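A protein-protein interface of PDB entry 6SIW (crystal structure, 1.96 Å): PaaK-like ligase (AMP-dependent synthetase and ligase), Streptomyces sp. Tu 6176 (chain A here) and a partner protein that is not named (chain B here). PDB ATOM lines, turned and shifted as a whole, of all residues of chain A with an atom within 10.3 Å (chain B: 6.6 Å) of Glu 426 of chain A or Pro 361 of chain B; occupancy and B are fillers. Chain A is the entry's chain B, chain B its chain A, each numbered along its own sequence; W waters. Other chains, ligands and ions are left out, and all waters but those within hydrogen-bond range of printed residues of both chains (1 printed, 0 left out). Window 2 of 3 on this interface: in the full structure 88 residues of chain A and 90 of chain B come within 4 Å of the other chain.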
ATOM      1  N   ARG A 421       1.241  -6.042  12.559  1.00  0.00           N
ATOM      2  CA  ARG A 421       1.328  -6.143  14.028  1.00  0.00           C
ATOM      3  C   ARG A 421      -0.021  -6.640  14.538  1.00  0.00           C
ATOM      4  O   ARG A 421      -1.028  -6.335  13.908  1.00  0.00           O
ATOM      5  CB  ARG A 421       1.697  -4.787  14.639  1.00  0.00           C
ATOM      6  CG  ARG A 421       3.153  -4.403  14.426  1.00  0.00           C
ATOM      7  CD  ARG A 421       3.550  -3.229  15.301  1.00  0.00           C
ATOM      8  NE  ARG A 421       3.194  -3.455  16.686  1.00  0.00           N
ATOM      9  CZ  ARG A 421       2.799  -2.515  17.532  1.00  0.00           C
ATOM     10  NH1 ARG A 421       2.700  -1.253  17.143  1.00  0.00           N
ATOM     11  NH2 ARG A 421       2.484  -2.846  18.773  1.00  0.00           N
ATOM     12  N   LEU A 423      -0.660  -7.391  18.405  1.00  0.00           N
ATOM     13  CA  LEU A 423      -0.906  -6.874  19.778  1.00  0.00           C
ATOM     14  C   LEU A 423      -0.491  -5.397  19.853  1.00  0.00           C
ATOM     15  O   LEU A 423       0.653  -5.064  19.498  1.00  0.00           O
ATOM     16  CB  LEU A 423      -0.144  -7.717  20.803  1.00  0.00           C
ATOM     17  CG  LEU A 423      -0.334  -7.270  22.245  1.00  0.00           C
ATOM     18  CD1 LEU A 423      -1.815  -7.289  22.610  1.00  0.00           C
ATOM     19  CD2 LEU A 423       0.479  -8.142  23.197  1.00  0.00           C
ATOM     20  N   PHE A 424      -1.395  -4.541  20.317  1.00  0.00           N
ATOM     21  CA  PHE A 424      -1.200  -3.074  20.405  1.00  0.00           C
ATOM     22  C   PHE A 424      -1.330  -2.618  21.853  1.00  0.00           C
ATOM     23  O   PHE A 424      -2.099  -3.225  22.623  1.00  0.00           O
ATOM     24  CB  PHE A 424      -2.220  -2.374  19.512  1.00  0.00           C
ATOM     25  CG  PHE A 424      -1.992  -2.647  18.055  1.00  0.00           C
ATOM     26  CD1 PHE A 424      -2.521  -3.776  17.456  1.00  0.00           C
ATOM     27  CD2 PHE A 424      -1.214  -1.787  17.295  1.00  0.00           C
ATOM     28  CE1 PHE A 424      -2.285  -4.030  16.110  1.00  0.00           C
ATOM     29  CE2 PHE A 424      -0.986  -2.040  15.954  1.00  0.00           C
ATOM     30  CZ  PHE A 424      -1.520  -3.159  15.364  1.00  0.00           C
ATOM     31  N   ALA A 425      -0.576  -1.577  22.198  1.00  0.00           N
ATOM     32  CA  ALA A 425      -0.726  -0.821  23.464  1.00  0.00           C
ATOM     33  C   ALA A 425      -1.975   0.051  23.343  1.00  0.00           C
ATOM     34  O   ALA A 425      -2.332   0.403  22.197  1.00  0.00           O
ATOM     35  CB  ALA A 425       0.510   0.003  23.734  1.00  0.00           C
ATOM     36  N   GLU A 426      -2.591   0.384  24.479  1.00  0.00           N
ATOM     37  CA  GLU A 426      -3.868   1.143  24.575  1.00  0.00           C
ATOM     38  C   GLU A 426      -3.851   2.369  23.647  1.00  0.00           C
ATOM     39  O   GLU A 426      -4.887   2.628  22.994  1.00  0.00           O
ATOM     40  CB  GLU A 426      -4.112   1.559  26.025  1.00  0.00           C
ATOM     41  CG  GLU A 426      -5.254   2.548  26.168  1.00  0.00           C
ATOM     42  CD  GLU A 426      -5.928   2.556  27.521  1.00  0.00           C
ATOM     43  OE1 GLU A 426      -6.455   1.502  27.921  1.00  0.00           O
ATOM     44  OE2 GLU A 426      -5.915   3.612  28.159  1.00  0.00           O
ATOM     45  N   ASP A 427      -2.720   3.080  23.585  1.00  0.00           N
ATOM     46  CA  ASP A 427      -2.590   4.408  22.924  1.00  0.00           C
ATOM     47  C   ASP A 427      -2.269   4.280  21.425  1.00  0.00           C
ATOM     48  O   ASP A 427      -2.092   5.339  20.791  1.00  0.00           O
ATOM     49  CB  ASP A 427      -1.509   5.246  23.610  1.00  0.00           C
ATOM     50  CG  ASP A 427      -0.125   4.627  23.538  1.00  0.00           C
ATOM     51  OD1 ASP A 427       0.043   3.509  24.062  1.00  0.00           O
ATOM     52  OD2 ASP A 427       0.768   5.258  22.953  1.00  0.00           O
ATOM     53  N   GLU A 428      -2.189   3.064  20.865  1.00  0.00           N
ATOM     54  CA  GLU A 428      -1.798   2.857  19.443  1.00  0.00           C
ATOM     55  C   GLU A 428      -3.046   2.675  18.574  1.00  0.00           C
ATOM     56  O   GLU A 428      -4.098   2.300  19.113  1.00  0.00           O
ATOM     57  CB  GLU A 428      -0.874   1.653  19.293  1.00  0.00           C
ATOM     58  CG  GLU A 428       0.417   1.775  20.075  1.00  0.00           C
ATOM     59  CD  GLU A 428       1.429   0.703  19.726  1.00  0.00           C
ATOM     60  OE1 GLU A 428       1.490  -0.320  20.435  1.00  0.00           O
ATOM     61  OE2 GLU A 428       2.131   0.880  18.722  1.00  0.00           O
ATOM     62  N   ASP A 429      -2.917   2.938  17.273  1.00  0.00           N
ATOM     63  CA  ASP A 429      -4.002   2.757  16.273  1.00  0.00           C
ATOM     64  C   ASP A 429      -3.939   1.324  15.743  1.00  0.00           C
ATOM     65  O   ASP A 429      -3.099   1.059  14.861  1.00  0.00           O
ATOM     66  CB  ASP A 429      -3.920   3.784  15.143  1.00  0.00           C
ATOM     67  CG  ASP A 429      -5.243   3.956  14.414  1.00  0.00           C
ATOM     68  OD1 ASP A 429      -5.995   2.959  14.315  1.00  0.00           O
ATOM     69  OD2 ASP A 429      -5.530   5.092  13.981  1.00  0.00           O
ATOM     70  N   TRP A 430      -4.812   0.437  16.238  1.00  0.00           N
ATOM     71  CA  TRP A 430      -4.814  -0.997  15.841  1.00  0.00           C
ATOM     72  C   TRP A 430      -5.561  -1.235  14.517  1.00  0.00           C
ATOM     73  O   TRP A 430      -5.729  -2.403  14.152  1.00  0.00           O
ATOM     74  CB  TRP A 430      -5.328  -1.884  16.984  1.00  0.00           C
ATOM     75  CG  TRP A 430      -6.808  -1.882  17.203  1.00  0.00           C
ATOM     76  CD1 TRP A 430      -7.706  -0.920  16.837  1.00  0.00           C
ATOM     77  CD2 TRP A 430      -7.560  -2.896  17.888  1.00  0.00           C
ATOM     78  NE1 TRP A 430      -8.968  -1.276  17.235  1.00  0.00           N
ATOM     79  CE2 TRP A 430      -8.909  -2.478  17.889  1.00  0.00           C
ATOM     80  CE3 TRP A 430      -7.229  -4.111  18.495  1.00  0.00           C
ATOM     81  CZ2 TRP A 430      -9.923  -3.244  18.463  1.00  0.00           C
ATOM     82  CZ3 TRP A 430      -8.231  -4.858  19.073  1.00  0.00           C
ATOM     83  CH2 TRP A 430      -9.559  -4.431  19.053  1.00  0.00           C
ATOM     84  N   ASP A 431      -5.949  -0.178  13.801  1.00  0.00           N
ATOM     85  CA  ASP A 431      -6.599  -0.293  12.468  1.00  0.00           C
ATOM     86  C   ASP A 431      -5.528  -0.520  11.384  1.00  0.00           C
ATOM     87  O   ASP A 431      -5.936  -0.584  10.200  1.00  0.00           O
ATOM     88  CB  ASP A 431      -7.533   0.897  12.203  1.00  0.00           C
ATOM     89  CG  ASP A 431      -8.782   0.885  13.078  1.00  0.00           C
ATOM     90  OD1 ASP A 431      -9.356  -0.199  13.246  1.00  0.00           O
ATOM     91  OD2 ASP A 431      -9.169   1.952  13.597  1.00  0.00           O
ATOM     92  N   HIS B 327       3.358  -6.573  27.710  1.00  0.00           N
ATOM     93  CA  HIS B 327       2.329  -5.633  28.223  1.00  0.00           C
ATOM     94  C   HIS B 327       1.721  -6.222  29.490  1.00  0.00           C
ATOM     95  O   HIS B 327       1.371  -7.429  29.484  1.00  0.00           O
ATOM     96  CB  HIS B 327       1.245  -5.371  27.189  1.00  0.00           C
ATOM     97  CG  HIS B 327       1.761  -4.901  25.877  1.00  0.00           C
ATOM     98  ND1 HIS B 327       1.693  -3.575  25.503  1.00  0.00           N
ATOM     99  CD2 HIS B 327       2.310  -5.565  24.836  1.00  0.00           C
ATOM    100  CE1 HIS B 327       2.172  -3.440  24.282  1.00  0.00           C
ATOM    101  NE2 HIS B 327       2.564  -4.649  23.851  1.00  0.00           N
ATOM    102  N   ARG B 328       1.607  -5.401  30.532  1.00  0.00           N
ATOM    103  CA  ARG B 328       1.010  -5.798  31.832  1.00  0.00           C
ATOM    104  C   ARG B 328      -0.495  -5.521  31.735  1.00  0.00           C
ATOM    105  O   ARG B 328      -0.867  -4.404  31.328  1.00  0.00           O
ATOM    106  CB  ARG B 328       1.749  -5.075  32.968  1.00  0.00           C
ATOM    107  CG  ARG B 328       1.123  -5.180  34.356  1.00  0.00           C
ATOM    108  CD  ARG B 328       0.923  -6.584  34.895  1.00  0.00           C
ATOM    109  NE  ARG B 328       2.105  -7.233  35.457  1.00  0.00           N
ATOM    110  CZ  ARG B 328       2.537  -7.097  36.713  1.00  0.00           C
ATOM    111  NH1 ARG B 328       1.910  -6.298  37.563  1.00  0.00           N
ATOM    112  NH2 ARG B 328       3.609  -7.762  37.115  1.00  0.00           N
ATOM    113  N   ILE B 329      -1.311  -6.553  31.945  1.00  0.00           N
ATOM    114  CA  ILE B 329      -2.795  -6.493  31.834  1.00  0.00           C
ATOM    115  C   ILE B 329      -3.351  -7.123  33.106  1.00  0.00           C
ATOM    116  O   ILE B 329      -3.380  -8.370  33.157  1.00  0.00           O
ATOM    117  CB  ILE B 329      -3.303  -7.213  30.571  1.00  0.00           C
ATOM    118  CG1 ILE B 329      -2.699  -6.639  29.290  1.00  0.00           C
ATOM    119  CG2 ILE B 329      -4.819  -7.190  30.514  1.00  0.00           C
ATOM    120  CD1 ILE B 329      -2.989  -7.494  28.082  1.00  0.00           C
ATOM    121  N   GLY B 330      -3.754  -6.301  34.081  1.00  0.00           N
ATOM    122  CA  GLY B 330      -4.107  -6.779  35.434  1.00  0.00           C
ATOM    123  C   GLY B 330      -2.919  -7.510  36.053  1.00  0.00           C
ATOM    124  O   GLY B 330      -1.826  -6.951  36.074  1.00  0.00           O
ATOM    125  N   PRO B 331      -3.061  -8.790  36.481  1.00  0.00           N
ATOM    126  CA  PRO B 331      -1.967  -9.517  37.127  1.00  0.00           C
ATOM    127  C   PRO B 331      -0.861  -9.980  36.161  1.00  0.00           C
ATOM    128  O   PRO B 331       0.279 -10.054  36.577  1.00  0.00           O
ATOM    129  CB  PRO B 331      -2.679 -10.741  37.725  1.00  0.00           C
ATOM    130  CG  PRO B 331      -3.812 -11.006  36.756  1.00  0.00           C
ATOM    131  CD  PRO B 331      -4.258  -9.630  36.301  1.00  0.00           C
ATOM    132  N   LYS B 358      -5.633  -5.452  21.753  1.00  0.00           N
ATOM    133  CA  LYS B 358      -5.167  -4.233  22.449  1.00  0.00           C
ATOM    134  C   LYS B 358      -4.941  -4.584  23.922  1.00  0.00           C
ATOM    135  O   LYS B 358      -5.878  -5.115  24.566  1.00  0.00           O
ATOM    136  CB  LYS B 358      -6.184  -3.096  22.301  1.00  0.00           C
ATOM    137  CG  LYS B 358      -5.637  -1.712  22.641  1.00  0.00           C
ATOM    138  CD  LYS B 358      -6.548  -0.593  22.221  1.00  0.00           C
ATOM    139  CE  LYS B 358      -6.519  -0.337  20.730  1.00  0.00           C
ATOM    140  NZ  LYS B 358      -7.861   0.031  20.220  1.00  0.00           N
ATOM    141  N   ALA B 359      -3.732  -4.318  24.411  1.00  0.00           N
ATOM    142  CA  ALA B 359      -3.368  -4.388  25.838  1.00  0.00           C
ATOM    143  C   ALA B 359      -3.866  -3.120  26.543  1.00  0.00           C
ATOM    144  O   ALA B 359      -3.193  -2.085  26.438  1.00  0.00           O
ATOM    145  CB  ALA B 359      -1.877  -4.549  25.964  1.00  0.00           C
ATOM    146  N   HIS B 360      -5.024  -3.195  27.196  1.00  0.00           N
ATOM    147  CA  HIS B 360      -5.486  -2.176  28.172  1.00  0.00           C
ATOM    148  C   HIS B 360      -4.883  -2.501  29.536  1.00  0.00           C
ATOM    149  O   HIS B 360      -4.548  -3.655  29.812  1.00  0.00           O
ATOM    150  CB  HIS B 360      -7.013  -2.115  28.250  1.00  0.00           C
ATOM    151  CG  HIS B 360      -7.698  -1.887  26.952  1.00  0.00           C
ATOM    152  ND1 HIS B 360      -7.869  -0.627  26.426  1.00  0.00           N
ATOM    153  CD2 HIS B 360      -8.300  -2.745  26.104  1.00  0.00           C
ATOM    154  CE1 HIS B 360      -8.542  -0.713  25.297  1.00  0.00           C
ATOM    155  NE2 HIS B 360      -8.817  -2.006  25.076  1.00  0.00           N
ATOM    156  N   PRO B 361      -4.744  -1.500  30.438  1.00  0.00           N
ATOM    157  CA  PRO B 361      -4.241  -1.755  31.787  1.00  0.00           C
ATOM    158  C   PRO B 361      -5.035  -2.844  32.532  1.00  0.00           C
ATOM    159  O   PRO B 361      -4.455  -3.535  33.334  1.00  0.00           O
ATOM    160  CB  PRO B 361      -4.411  -0.406  32.503  1.00  0.00           C
ATOM    161  CG  PRO B 361      -4.433   0.626  31.399  1.00  0.00           C
ATOM    162  CD  PRO B 361      -5.035  -0.075  30.200  1.00  0.00           C
ATOM    163  N   ASP B 362      -6.331  -2.969  32.240  1.00  0.00           N
ATOM    164  CA  ASP B 362      -7.285  -3.819  33.002  1.00  0.00           C
ATOM    165  C   ASP B 362      -7.652  -5.099  32.234  1.00  0.00           C
ATOM    166  O   ASP B 362      -8.058  -6.060  32.888  1.00  0.00           O
ATOM    167  CB  ASP B 362      -8.547  -3.032  33.363  1.00  0.00           C
ATOM    168  CG  ASP B 362      -9.202  -2.305  32.197  1.00  0.00           C
ATOM    169  OD1 ASP B 362      -8.477  -1.847  31.291  1.00  0.00           O
ATOM    170  OD2 ASP B 362     -10.438  -2.177  32.220  1.00  0.00           O
ATOM    171  N   VAL B 363      -7.536  -5.131  30.905  1.00  0.00           N
ATOM    172  CA  VAL B 363      -8.228  -6.169  30.085  1.00  0.00           C
ATOM    173  C   VAL B 363      -7.559  -6.288  28.707  1.00  0.00           C
ATOM    174  O   VAL B 363      -7.066  -5.282  28.174  1.00  0.00           O
ATOM    175  CB  VAL B 363      -9.738  -5.857  29.982  1.00  0.00           C
ATOM    176  CG1 VAL B 363     -10.031  -4.690  29.053  1.00  0.00           C
ATOM    177  CG2 VAL B 363     -10.544  -7.065  29.539  1.00  0.00           C
HETATM  178  O   HOH W   1      -6.237   1.863  18.077  1.00  0.00           O
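A ring nitrogen (ND1) of His 360 of chain B is in hydrogen-bond range of the side-chain carboxylate (OE1) of Glu 426 of chain A (3.0 Å). O of Phe 424 of chain A sits at hydrogen-bond distance from N of Ala 359 of chain B, at 2.7 Å. The backbone carbonyl oxygen (O) of Ala 359 of chain B lies within hydrogen-bond range of the backbone NH (N) of Glu 426 of chain A. NZ of Lys 358 of chain B sits close to NE1 of Trp 430 of chain A, at 3.4 Å.
The backbone NH (N) of Ala 425 of chain A is in hydrogen-bond range of the side-chain carboxylate (OE1) of Glu 428 of chain A (3.0 Å). The guanidinium group (NH1) of Arg 421 of chain A is in salt-bridge range of the side-chain carboxylate (OE2) of Glu 428 of chain A (2.7 Å). The backbone carbonyl oxygen of Leu 423 of chain A lies within hydrogen-bond range of the guanidinium group of Arg 421 of chain A (3.0 Å). N of Gly 330 of chain B is in hydrogen-bond range of O of Pro 361 of chain B (2.9 Å).
Among the printed residues, pairs that only touch across the chains: Leu 423 of chain A with His 327 of chain B (3.6 Å), Leu 423 of chain A with Ala 359 of chain B (3.97 Å), Phe 424 of chain A with Lys 358 of chain B (3.2 Å), Ala 425 of chain A with His 327 of chain B (3.9 Å), Ala 425 of chain A with Lys 358 of chain B (3.9 Å), Ala 425 of chain A with Ala 359 of chain B (3.95 Å), Glu 426 of chain A with Lys 358 of chain B (3.7 Å), Glu 426 of chain A with Pro 361 of chain B (3.1 Å) and Glu 428 of chain A with Lys 358 of chain B (3.9 Å).
Glu 426 of chain A touches just these residues of chain B: Lys 358 (3.7 Å), Ala 359 (3.2 Å), His 360 (3.0 Å) and Pro 361 (3.1 Å). Of chain A, only Glu 426 (3.1 Å) comes within 4 Å of Pro 361 of chain B. No residue of chain A comes within 4 Å of Gly 330 of chain B. Of the printed residues of chain A, Ala 359 of chain B touches Leu 423 (3.97 Å), Phe 424 (2.7 Å), Ala 425 (3.95 Å) and Glu 426 (3.2 Å). No residue of chain A comes within 4 Å of Asp 362 of chain B. Of the printed residues of chain B, Ala 425 of chain A touches His 327, Lys 358 and Ala 359. Of the printed residues of chain B, Glu 428 of chain A touches Lys 358. Printed residues of chain B within 4 Å of Leu 423 of chain A: His 327 and Ala 359. Printed residues of chain B within 4 Å of Trp 430 of chain A: Lys 358. Pro 331 of chain B touches none of the printed residues of chain A. Arg 328 of chain B touches none of the printed residues of chain A. The nearest residue of chain B that does not touch Glu 426 of chain A is Asp 362 of chain B (5.2 Å). The nearest residue of chain A that does not touch Pro 361 of chain B is Ala 425 of chain A (7.5 Å).
Printed residues of chain A that touch a printed residue of chain B: Leu 423, Phe 424, Ala 425, Glu 426, Glu 428 and Trp 430. Hydrophobic or aromatic side chains of chain A that line the printed part of chain B: Leu 423, Ala 425 and Trp 430. Along chain A the printed residues that touch a printed residue of chain B span positions 423 to 430. Printed residues of chain B that touch a printed residue of chain A: His 327, Lys 358, Ala 359, His 360 and Pro 361. Among the printed residues, no Asp or Glu carboxylate lies within 4 Å of a Lys or Arg side-chain nitrogen of the other chain.
Water W1 lies within hydrogen-bond range of the backbone carbonyl oxygen of Glu 428 of chain A (2.4 Å), the backbone NH of Trp 430 of chain A (2.7 Å) and the side-chain amino group of Lys 358 of chain B (3.3 Å).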
